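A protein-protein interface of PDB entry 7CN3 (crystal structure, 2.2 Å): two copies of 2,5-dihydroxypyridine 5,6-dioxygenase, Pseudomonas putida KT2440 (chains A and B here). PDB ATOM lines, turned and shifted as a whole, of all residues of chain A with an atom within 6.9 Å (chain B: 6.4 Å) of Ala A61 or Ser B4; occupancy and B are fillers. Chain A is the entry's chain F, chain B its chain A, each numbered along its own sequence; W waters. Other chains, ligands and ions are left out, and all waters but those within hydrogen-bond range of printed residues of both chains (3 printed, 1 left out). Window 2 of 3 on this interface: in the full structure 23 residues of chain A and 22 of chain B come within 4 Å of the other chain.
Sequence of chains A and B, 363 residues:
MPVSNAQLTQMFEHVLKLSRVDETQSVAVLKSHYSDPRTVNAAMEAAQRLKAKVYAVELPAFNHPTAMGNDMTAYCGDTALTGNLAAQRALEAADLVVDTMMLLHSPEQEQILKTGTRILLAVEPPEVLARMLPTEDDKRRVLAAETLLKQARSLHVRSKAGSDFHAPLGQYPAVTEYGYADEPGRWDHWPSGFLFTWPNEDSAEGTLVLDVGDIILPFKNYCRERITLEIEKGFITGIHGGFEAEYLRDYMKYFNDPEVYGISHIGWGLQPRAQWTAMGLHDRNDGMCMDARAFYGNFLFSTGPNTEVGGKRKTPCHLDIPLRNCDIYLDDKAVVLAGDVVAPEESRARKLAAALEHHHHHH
No position is printed for both chains. Of the 10 pairs that touch across the chains among the printed residues, none has its exchanged pair printed and touching as well.
The backbone carbonyl oxygen (O) of Pro B2 sits close to the backbone carbonyl oxygen (O) of Phe A62, at 2.9 Å. N of Pro B2 sits close to OD1 of Asn A63 (3.4 Å).
Ala A61 touches just these residues of chain B: Pro B2 and Ser B4. Of chain A, only Ala A61 (3.8 Å) comes within 4 Å of Ser B4. Printed residues of chain A within 4 Å of Pro B2: Tyr A34, Ala A61, Phe A62 and Asn A63. Of the printed residues of chain B, Tyr A34 touches Pro B2. Of the printed residues of chain B, His A33 touches Val B3 and Arg B38. Printed residues of chain B within 4 Å of Phe A62: Pro B2 (2.9 Å). Of the printed residues of chain B, Asn A63 touches Pro B2, Val B3, Gln B7 and Glu B127. The nearest residue of chain A that does not touch Ser B4 is Pro A60 (4.4 Å).
Of the 11 printed residues of chain B, 6 touch a printed residue of chain A. Printed residues of chain B that touch a printed residue of chain A: Pro B2, Val B3, Ser B4, Gln B7, Arg B38 and Glu B127. Hydrophobic or aromatic side chains of chain B within 4 Å of the printed part of chain A: Pro B2 and Val B3. Of the 11 printed residues of chain A, 5 touch a printed residue of chain B. Hydrophobic or aromatic side chains of chain A that line the printed part of chain B: His A33, Tyr A34 and Ala A61.
Water W3 lies within hydrogen-bond range of OE1 of Gln B7 (2.6 Å) and N of Asn A63 (2.8 Å). Water W2 lies within hydrogen-bond range of the side-chain amide nitrogen (ND2) of Asn A63 and the side-chain amide nitrogen (NE2) of Gln B7. Water W1 lies within hydrogen-bond range of O of Glu B127 (3.1 Å) and ND2 of Asn A63 (3.2 Å).
Among the printed residues, pairs that only touch across the chains: His A33 with Val B3 (3.2 Å), Ala A61 with Pro B2 (3.4 Å), His A33 with Arg B38 (3.5 Å), Tyr A34 with Pro B2 (3.5 Å), Asn A63 with Glu B127 (3.6 Å), Asn A63 with Val B3 (3.7 Å), Asn A63 with Gln B7 (3.7 Å) and Ala A61 with Ser B4 (3.8 Å).
The backbone carbonyl oxygen of Val B3 lies within hydrogen-bond range of the guanidinium group of Arg B38 (2.7 Å). OE2 of Glu B127 sits at hydrogen-bond distance from N of Val B3 (2.8 Å). The side-chain hydroxyl (OG) of Ser B4 lies within hydrogen-bond range of the backbone NH (N) of Gln B7, 3.0 Å away. NH2 of Arg B38 lies within hydrogen-bond range of OD1 of Asn B5. The side-chain hydroxyl of Ser A32 lies within hydrogen-bond range of the backbone NH of Ala A61, at 3.3 Å. O of Met A101 lies within hydrogen-bond range of OH of Tyr A34.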
ATOM      1  N   SER A  32      -2.773   0.231  35.941  1.00  0.00           N
ATOM      2  CA  SER A  32      -2.430   0.876  34.687  1.00  0.00           C
ATOM      3  C   SER A  32      -0.999   1.390  34.816  1.00  0.00           C
ATOM      4  O   SER A  32      -0.344   1.195  35.856  1.00  0.00           O
ATOM      5  CB  SER A  32      -3.424   1.998  34.374  1.00  0.00           C
ATOM      6  OG  SER A  32      -3.285   2.456  33.047  1.00  0.00           O
ATOM      7  N   HIS A  33      -0.512   2.086  33.776  1.00  0.00           N
ATOM      8  CA  HIS A  33       0.898   2.485  33.777  1.00  0.00           C
ATOM      9  C   HIS A  33       1.220   3.466  34.903  1.00  0.00           C
ATOM     10  O   HIS A  33       2.354   3.508  35.374  1.00  0.00           O
ATOM     11  CB  HIS A  33       1.309   3.098  32.428  1.00  0.00           C
ATOM     12  CG  HIS A  33       0.913   4.534  32.272  1.00  0.00           C
ATOM     13  ND1 HIS A  33      -0.254   4.921  31.645  1.00  0.00           N
ATOM     14  CD2 HIS A  33       1.526   5.679  32.666  1.00  0.00           C
ATOM     15  CE1 HIS A  33      -0.339   6.242  31.655  1.00  0.00           C
ATOM     16  NE2 HIS A  33       0.726   6.726  32.268  1.00  0.00           N
ATOM     17  N   TYR A  34       0.259   4.264  35.337  1.00  0.00           N
ATOM     18  CA  TYR A  34       0.504   5.246  36.384  1.00  0.00           C
ATOM     19  C   TYR A  34       0.245   4.713  37.799  1.00  0.00           C
ATOM     20  O   TYR A  34       0.346   5.485  38.756  1.00  0.00           O
ATOM     21  CB  TYR A  34      -0.360   6.487  36.130  1.00  0.00           C
ATOM     22  CG  TYR A  34      -1.830   6.151  36.049  1.00  0.00           C
ATOM     23  CD1 TYR A  34      -2.617   6.089  37.209  1.00  0.00           C
ATOM     24  CD2 TYR A  34      -2.426   5.857  34.825  1.00  0.00           C
ATOM     25  CE1 TYR A  34      -3.977   5.756  37.142  1.00  0.00           C
ATOM     26  CE2 TYR A  34      -3.770   5.533  34.743  1.00  0.00           C
ATOM     27  CZ  TYR A  34      -4.534   5.491  35.903  1.00  0.00           C
ATOM     28  OH  TYR A  34      -5.856   5.160  35.818  1.00  0.00           O
ATOM     29  N   LEU A  59      -4.650  -2.474  32.394  1.00  0.00           N
ATOM     30  CA  LEU A  59      -5.434  -1.807  31.355  1.00  0.00           C
ATOM     31  C   LEU A  59      -4.687  -0.603  30.806  1.00  0.00           C
ATOM     32  O   LEU A  59      -4.097   0.155  31.584  1.00  0.00           O
ATOM     33  CB  LEU A  59      -6.775  -1.312  31.895  1.00  0.00           C
ATOM     34  CG  LEU A  59      -7.808  -2.302  32.392  1.00  0.00           C
ATOM     35  CD1 LEU A  59      -8.964  -1.479  32.986  1.00  0.00           C
ATOM     36  CD2 LEU A  59      -8.238  -3.133  31.222  1.00  0.00           C
ATOM     37  N   PRO A  60      -4.719  -0.369  29.494  1.00  0.00           N
ATOM     38  CA  PRO A  60      -4.178   0.894  28.968  1.00  0.00           C
ATOM     39  C   PRO A  60      -4.928   2.091  29.559  1.00  0.00           C
ATOM     40  O   PRO A  60      -6.150   2.062  29.712  1.00  0.00           O
ATOM     41  CB  PRO A  60      -4.394   0.778  27.449  1.00  0.00           C
ATOM     42  CG  PRO A  60      -4.652  -0.718  27.204  1.00  0.00           C
ATOM     43  CD  PRO A  60      -5.338  -1.198  28.446  1.00  0.00           C
ATOM     44  N   ALA A  61      -4.172   3.130  29.928  1.00  0.00           N
ATOM     45  CA  ALA A  61      -4.762   4.358  30.459  1.00  0.00           C
ATOM     46  C   ALA A  61      -5.825   4.944  29.536  1.00  0.00           C
ATOM     47  O   ALA A  61      -5.706   4.917  28.312  1.00  0.00           O
ATOM     48  CB  ALA A  61      -3.675   5.407  30.703  1.00  0.00           C
ATOM     49  N   PHE A  62      -6.878   5.476  30.132  1.00  0.00           N
ATOM     50  CA  PHE A  62      -7.901   6.199  29.398  1.00  0.00           C
ATOM     51  C   PHE A  62      -7.704   7.684  29.658  1.00  0.00           C
ATOM     52  O   PHE A  62      -7.337   8.088  30.768  1.00  0.00           O
ATOM     53  CB  PHE A  62      -9.306   5.772  29.819  1.00  0.00           C
ATOM     54  CG  PHE A  62     -10.385   6.413  29.005  1.00  0.00           C
ATOM     55  CD1 PHE A  62     -10.724   5.912  27.764  1.00  0.00           C
ATOM     56  CD2 PHE A  62     -11.048   7.538  29.474  1.00  0.00           C
ATOM     57  CE1 PHE A  62     -11.724   6.512  27.003  1.00  0.00           C
ATOM     58  CE2 PHE A  62     -12.040   8.145  28.718  1.00  0.00           C
ATOM     59  CZ  PHE A  62     -12.378   7.630  27.481  1.00  0.00           C
ATOM     60  N   ASN A  63      -7.896   8.497  28.626  1.00  0.00           N
ATOM     61  CA  ASN A  63      -7.624   9.918  28.771  1.00  0.00           C
ATOM     62  C   ASN A  63      -8.823  10.733  28.318  1.00  0.00           C
ATOM     63  O   ASN A  63      -9.390  10.488  27.251  1.00  0.00           O
ATOM     64  CB  ASN A  63      -6.377  10.354  28.009  1.00  0.00           C
ATOM     65  CG  ASN A  63      -5.930  11.730  28.425  1.00  0.00           C
ATOM     66  OD1 ASN A  63      -5.525  11.936  29.568  1.00  0.00           O
ATOM     67  ND2 ASN A  63      -6.049  12.697  27.516  1.00  0.00           N
ATOM     68  N   THR A  79     -14.162   5.343  31.728  1.00  0.00           N
ATOM     69  CA  THR A  79     -12.933   4.816  32.327  1.00  0.00           C
ATOM     70  C   THR A  79     -12.232   3.904  31.317  1.00  0.00           C
ATOM     71  O   THR A  79     -12.732   3.648  30.214  1.00  0.00           O
ATOM     72  CB  THR A  79     -13.222   4.034  33.623  1.00  0.00           C
ATOM     73  OG1 THR A  79     -13.999   2.864  33.318  1.00  0.00           O
ATOM     74  CG2 THR A  79     -13.979   4.895  34.648  1.00  0.00           C
ATOM     75  N   ALA A  80     -11.084   3.364  31.736  1.00  0.00           N
ATOM     76  CA  ALA A  80     -10.401   2.357  30.932  1.00  0.00           C
ATOM     77  C   ALA A  80     -11.238   1.103  30.732  1.00  0.00           C
ATOM     78  O   ALA A  80     -10.986   0.351  29.784  1.00  0.00           O
ATOM     79  CB  ALA A  80      -9.054   2.002  31.570  1.00  0.00           C
ATOM     80  N   MET A 101      -5.991   1.890  40.264  1.00  0.00           N
ATOM     81  CA  MET A 101      -6.011   2.822  39.143  1.00  0.00           C
ATOM     82  C   MET A 101      -7.229   3.736  39.139  1.00  0.00           C
ATOM     83  O   MET A 101      -7.259   4.668  38.329  1.00  0.00           O
ATOM     84  CB  MET A 101      -5.921   2.062  37.797  1.00  0.00           C
ATOM     85  CG  MET A 101      -7.247   1.490  37.307  1.00  0.00           C
ATOM     86  SD  MET A 101      -7.054   0.736  35.672  1.00  0.00           S
ATOM     87  CE  MET A 101      -7.191   2.185  34.634  1.00  0.00           C
ATOM     88  N   PRO B   2      -5.250   9.864  32.194  1.00  0.00           N
ATOM     89  CA  PRO B   2      -3.840   9.811  31.789  1.00  0.00           C
ATOM     90  C   PRO B   2      -3.688   9.249  30.382  1.00  0.00           C
ATOM     91  O   PRO B   2      -4.611   8.559  29.914  1.00  0.00           O
ATOM     92  CB  PRO B   2      -3.202   8.882  32.823  1.00  0.00           C
ATOM     93  CG  PRO B   2      -4.094   8.980  34.022  1.00  0.00           C
ATOM     94  CD  PRO B   2      -5.482   9.219  33.497  1.00  0.00           C
ATOM     95  N   VAL B   3      -2.549   9.522  29.734  1.00  0.00           N
ATOM     96  CA  VAL B   3      -2.324   9.169  28.332  1.00  0.00           C
ATOM     97  C   VAL B   3      -1.547   7.862  28.266  1.00  0.00           C
ATOM     98  O   VAL B   3      -0.485   7.742  28.879  1.00  0.00           O
ATOM     99  CB  VAL B   3      -1.572  10.283  27.580  1.00  0.00           C
ATOM    100  CG1 VAL B   3      -1.303   9.828  26.161  1.00  0.00           C
ATOM    101  CG2 VAL B   3      -2.369  11.590  27.564  1.00  0.00           C
ATOM    102  N   SER B   4      -2.060   6.884  27.508  1.00  0.00           N
ATOM    103  CA  SER B   4      -1.330   5.632  27.334  1.00  0.00           C
ATOM    104  C   SER B   4      -0.184   5.814  26.343  1.00  0.00           C
ATOM    105  O   SER B   4      -0.155   6.768  25.563  1.00  0.00           O
ATOM    106  CB  SER B   4      -2.245   4.513  26.833  1.00  0.00           C
ATOM    107  OG  SER B   4      -2.693   4.800  25.529  1.00  0.00           O
ATOM    108  N   ASN B   5       0.775   4.880  26.407  1.00  0.00           N
ATOM    109  CA  ASN B   5       1.864   4.819  25.429  1.00  0.00           C
ATOM    110  C   ASN B   5       1.329   4.760  24.008  1.00  0.00           C
ATOM    111  O   ASN B   5       1.853   5.430  23.111  1.00  0.00           O
ATOM    112  CB  ASN B   5       2.747   3.590  25.668  1.00  0.00           C
ATOM    113  CG  ASN B   5       3.665   3.744  26.843  1.00  0.00           C
ATOM    114  OD1 ASN B   5       3.587   4.715  27.594  1.00  0.00           O
ATOM    115  ND2 ASN B   5       4.546   2.770  27.019  1.00  0.00           N
ATOM    116  N   ALA B   6       0.320   3.925  23.770  1.00  0.00           N
ATOM    117  CA  ALA B   6      -0.254   3.860  22.434  1.00  0.00           C
ATOM    118  C   ALA B   6      -0.825   5.208  22.024  1.00  0.00           C
ATOM    119  O   ALA B   6      -0.596   5.672  20.902  1.00  0.00           O
ATOM    120  CB  ALA B   6      -1.340   2.779  22.359  1.00  0.00           C
ATOM    121  N   GLN B   7      -1.550   5.865  22.929  1.00  0.00           N
ATOM    122  CA  GLN B   7      -2.124   7.156  22.579  1.00  0.00           C
ATOM    123  C   GLN B   7      -1.029   8.200  22.364  1.00  0.00           C
ATOM    124  O   GLN B   7      -1.127   9.036  21.457  1.00  0.00           O
ATOM    125  CB  GLN B   7      -3.111   7.605  23.652  1.00  0.00           C
ATOM    126  CG  GLN B   7      -3.692   8.972  23.356  1.00  0.00           C
ATOM    127  CD  GLN B   7      -4.871   9.349  24.231  1.00  0.00           C
ATOM    128  OE1 GLN B   7      -5.484   8.504  24.886  1.00  0.00           O
ATOM    129  NE2 GLN B   7      -5.204  10.632  24.230  1.00  0.00           N
ATOM    130  N   LEU B   8       0.033   8.145  23.168  1.00  0.00           N
ATOM    131  CA  LEU B   8       1.108   9.127  23.051  1.00  0.00           C
ATOM    132  C   LEU B   8       1.808   9.026  21.691  1.00  0.00           C
ATOM    133  O   LEU B   8       2.071  10.042  21.040  1.00  0.00           O
ATOM    134  CB  LEU B   8       2.109   8.942  24.197  1.00  0.00           C
ATOM    135  CG  LEU B   8       3.132  10.073  24.421  1.00  0.00           C
ATOM    136  CD1 LEU B   8       2.451  11.445  24.431  1.00  0.00           C
ATOM    137  CD2 LEU B   8       3.936   9.860  25.698  1.00  0.00           C
ATOM    138  N   THR B   9       2.082   7.807  21.239  1.00  0.00           N
ATOM    139  CA  THR B   9       2.678   7.605  19.922  1.00  0.00           C
ATOM    140  C   THR B   9       1.768   8.099  18.790  1.00  0.00           C
ATOM    141  O   THR B   9       2.249   8.716  17.832  1.00  0.00           O
ATOM    142  CB  THR B   9       3.000   6.125  19.728  1.00  0.00           C
ATOM    143  OG1 THR B   9       4.015   5.730  20.656  1.00  0.00           O
ATOM    144  CG2 THR B   9       3.500   5.888  18.313  1.00  0.00           C
ATOM    145  N   MET B  11      -0.403  10.451  19.008  1.00  0.00           N
ATOM    146  CA  MET B  11      -0.422  11.905  19.070  1.00  0.00           C
ATOM    147  C   MET B  11       0.778  12.484  18.335  1.00  0.00           C
ATOM    148  O   MET B  11       0.647  13.447  17.576  1.00  0.00           O
ATOM    149  CB  MET B  11      -0.437  12.362  20.525  1.00  0.00           C
ATOM    150  CG  MET B  11      -1.832  12.498  21.135  1.00  0.00           C
ATOM    151  SD  MET B  11      -1.756  12.216  22.927  1.00  0.00           S
ATOM    152  CE  MET B  11      -0.454  13.319  23.460  1.00  0.00           C
ATOM    153  N   ARG B  38       9.008   8.510  28.184  1.00  0.00           N
ATOM    154  CA  ARG B  38       7.815   8.129  27.433  1.00  0.00           C
ATOM    155  C   ARG B  38       7.628   9.003  26.195  1.00  0.00           C
ATOM    156  O   ARG B  38       7.232   8.509  25.134  1.00  0.00           O
ATOM    157  CB  ARG B  38       6.588   8.213  28.343  1.00  0.00           C
ATOM    158  CG  ARG B  38       6.662   7.202  29.454  1.00  0.00           C
ATOM    159  CD  ARG B  38       5.428   7.259  30.301  1.00  0.00           C
ATOM    160  NE  ARG B  38       4.271   6.759  29.573  1.00  0.00           N
ATOM    161  CZ  ARG B  38       3.099   7.376  29.550  1.00  0.00           C
ATOM    162  NH1 ARG B  38       2.951   8.516  30.228  1.00  0.00           N
ATOM    163  NH2 ARG B  38       2.082   6.843  28.869  1.00  0.00           N
ATOM    164  N   GLU B 127      -0.569  14.510  29.256  1.00  0.00           N
ATOM    165  CA  GLU B 127      -1.972  14.904  29.325  1.00  0.00           C
ATOM    166  C   GLU B 127      -2.161  16.334  28.835  1.00  0.00           C
ATOM    167  O   GLU B 127      -3.184  16.662  28.222  1.00  0.00           O
ATOM    168  CB  GLU B 127      -2.505  14.738  30.752  1.00  0.00           C
ATOM    169  CG  GLU B 127      -2.572  13.267  31.216  1.00  0.00           C
ATOM    170  CD  GLU B 127      -1.188  12.652  31.412  1.00  0.00           C
ATOM    171  OE1 GLU B 127      -0.239  13.414  31.740  1.00  0.00           O
ATOM    172  OE2 GLU B 127      -1.049  11.420  31.226  1.00  0.00           O
HETATM  173  O   HOH W   1      -6.081  15.741  28.578  1.00  0.00           O
HETATM  174  O   HOH W   2      -6.828  12.605  25.001  1.00  0.00           O
HETATM  175  O   HOH W   3      -7.680   7.577  26.000  1.00  0.00           O
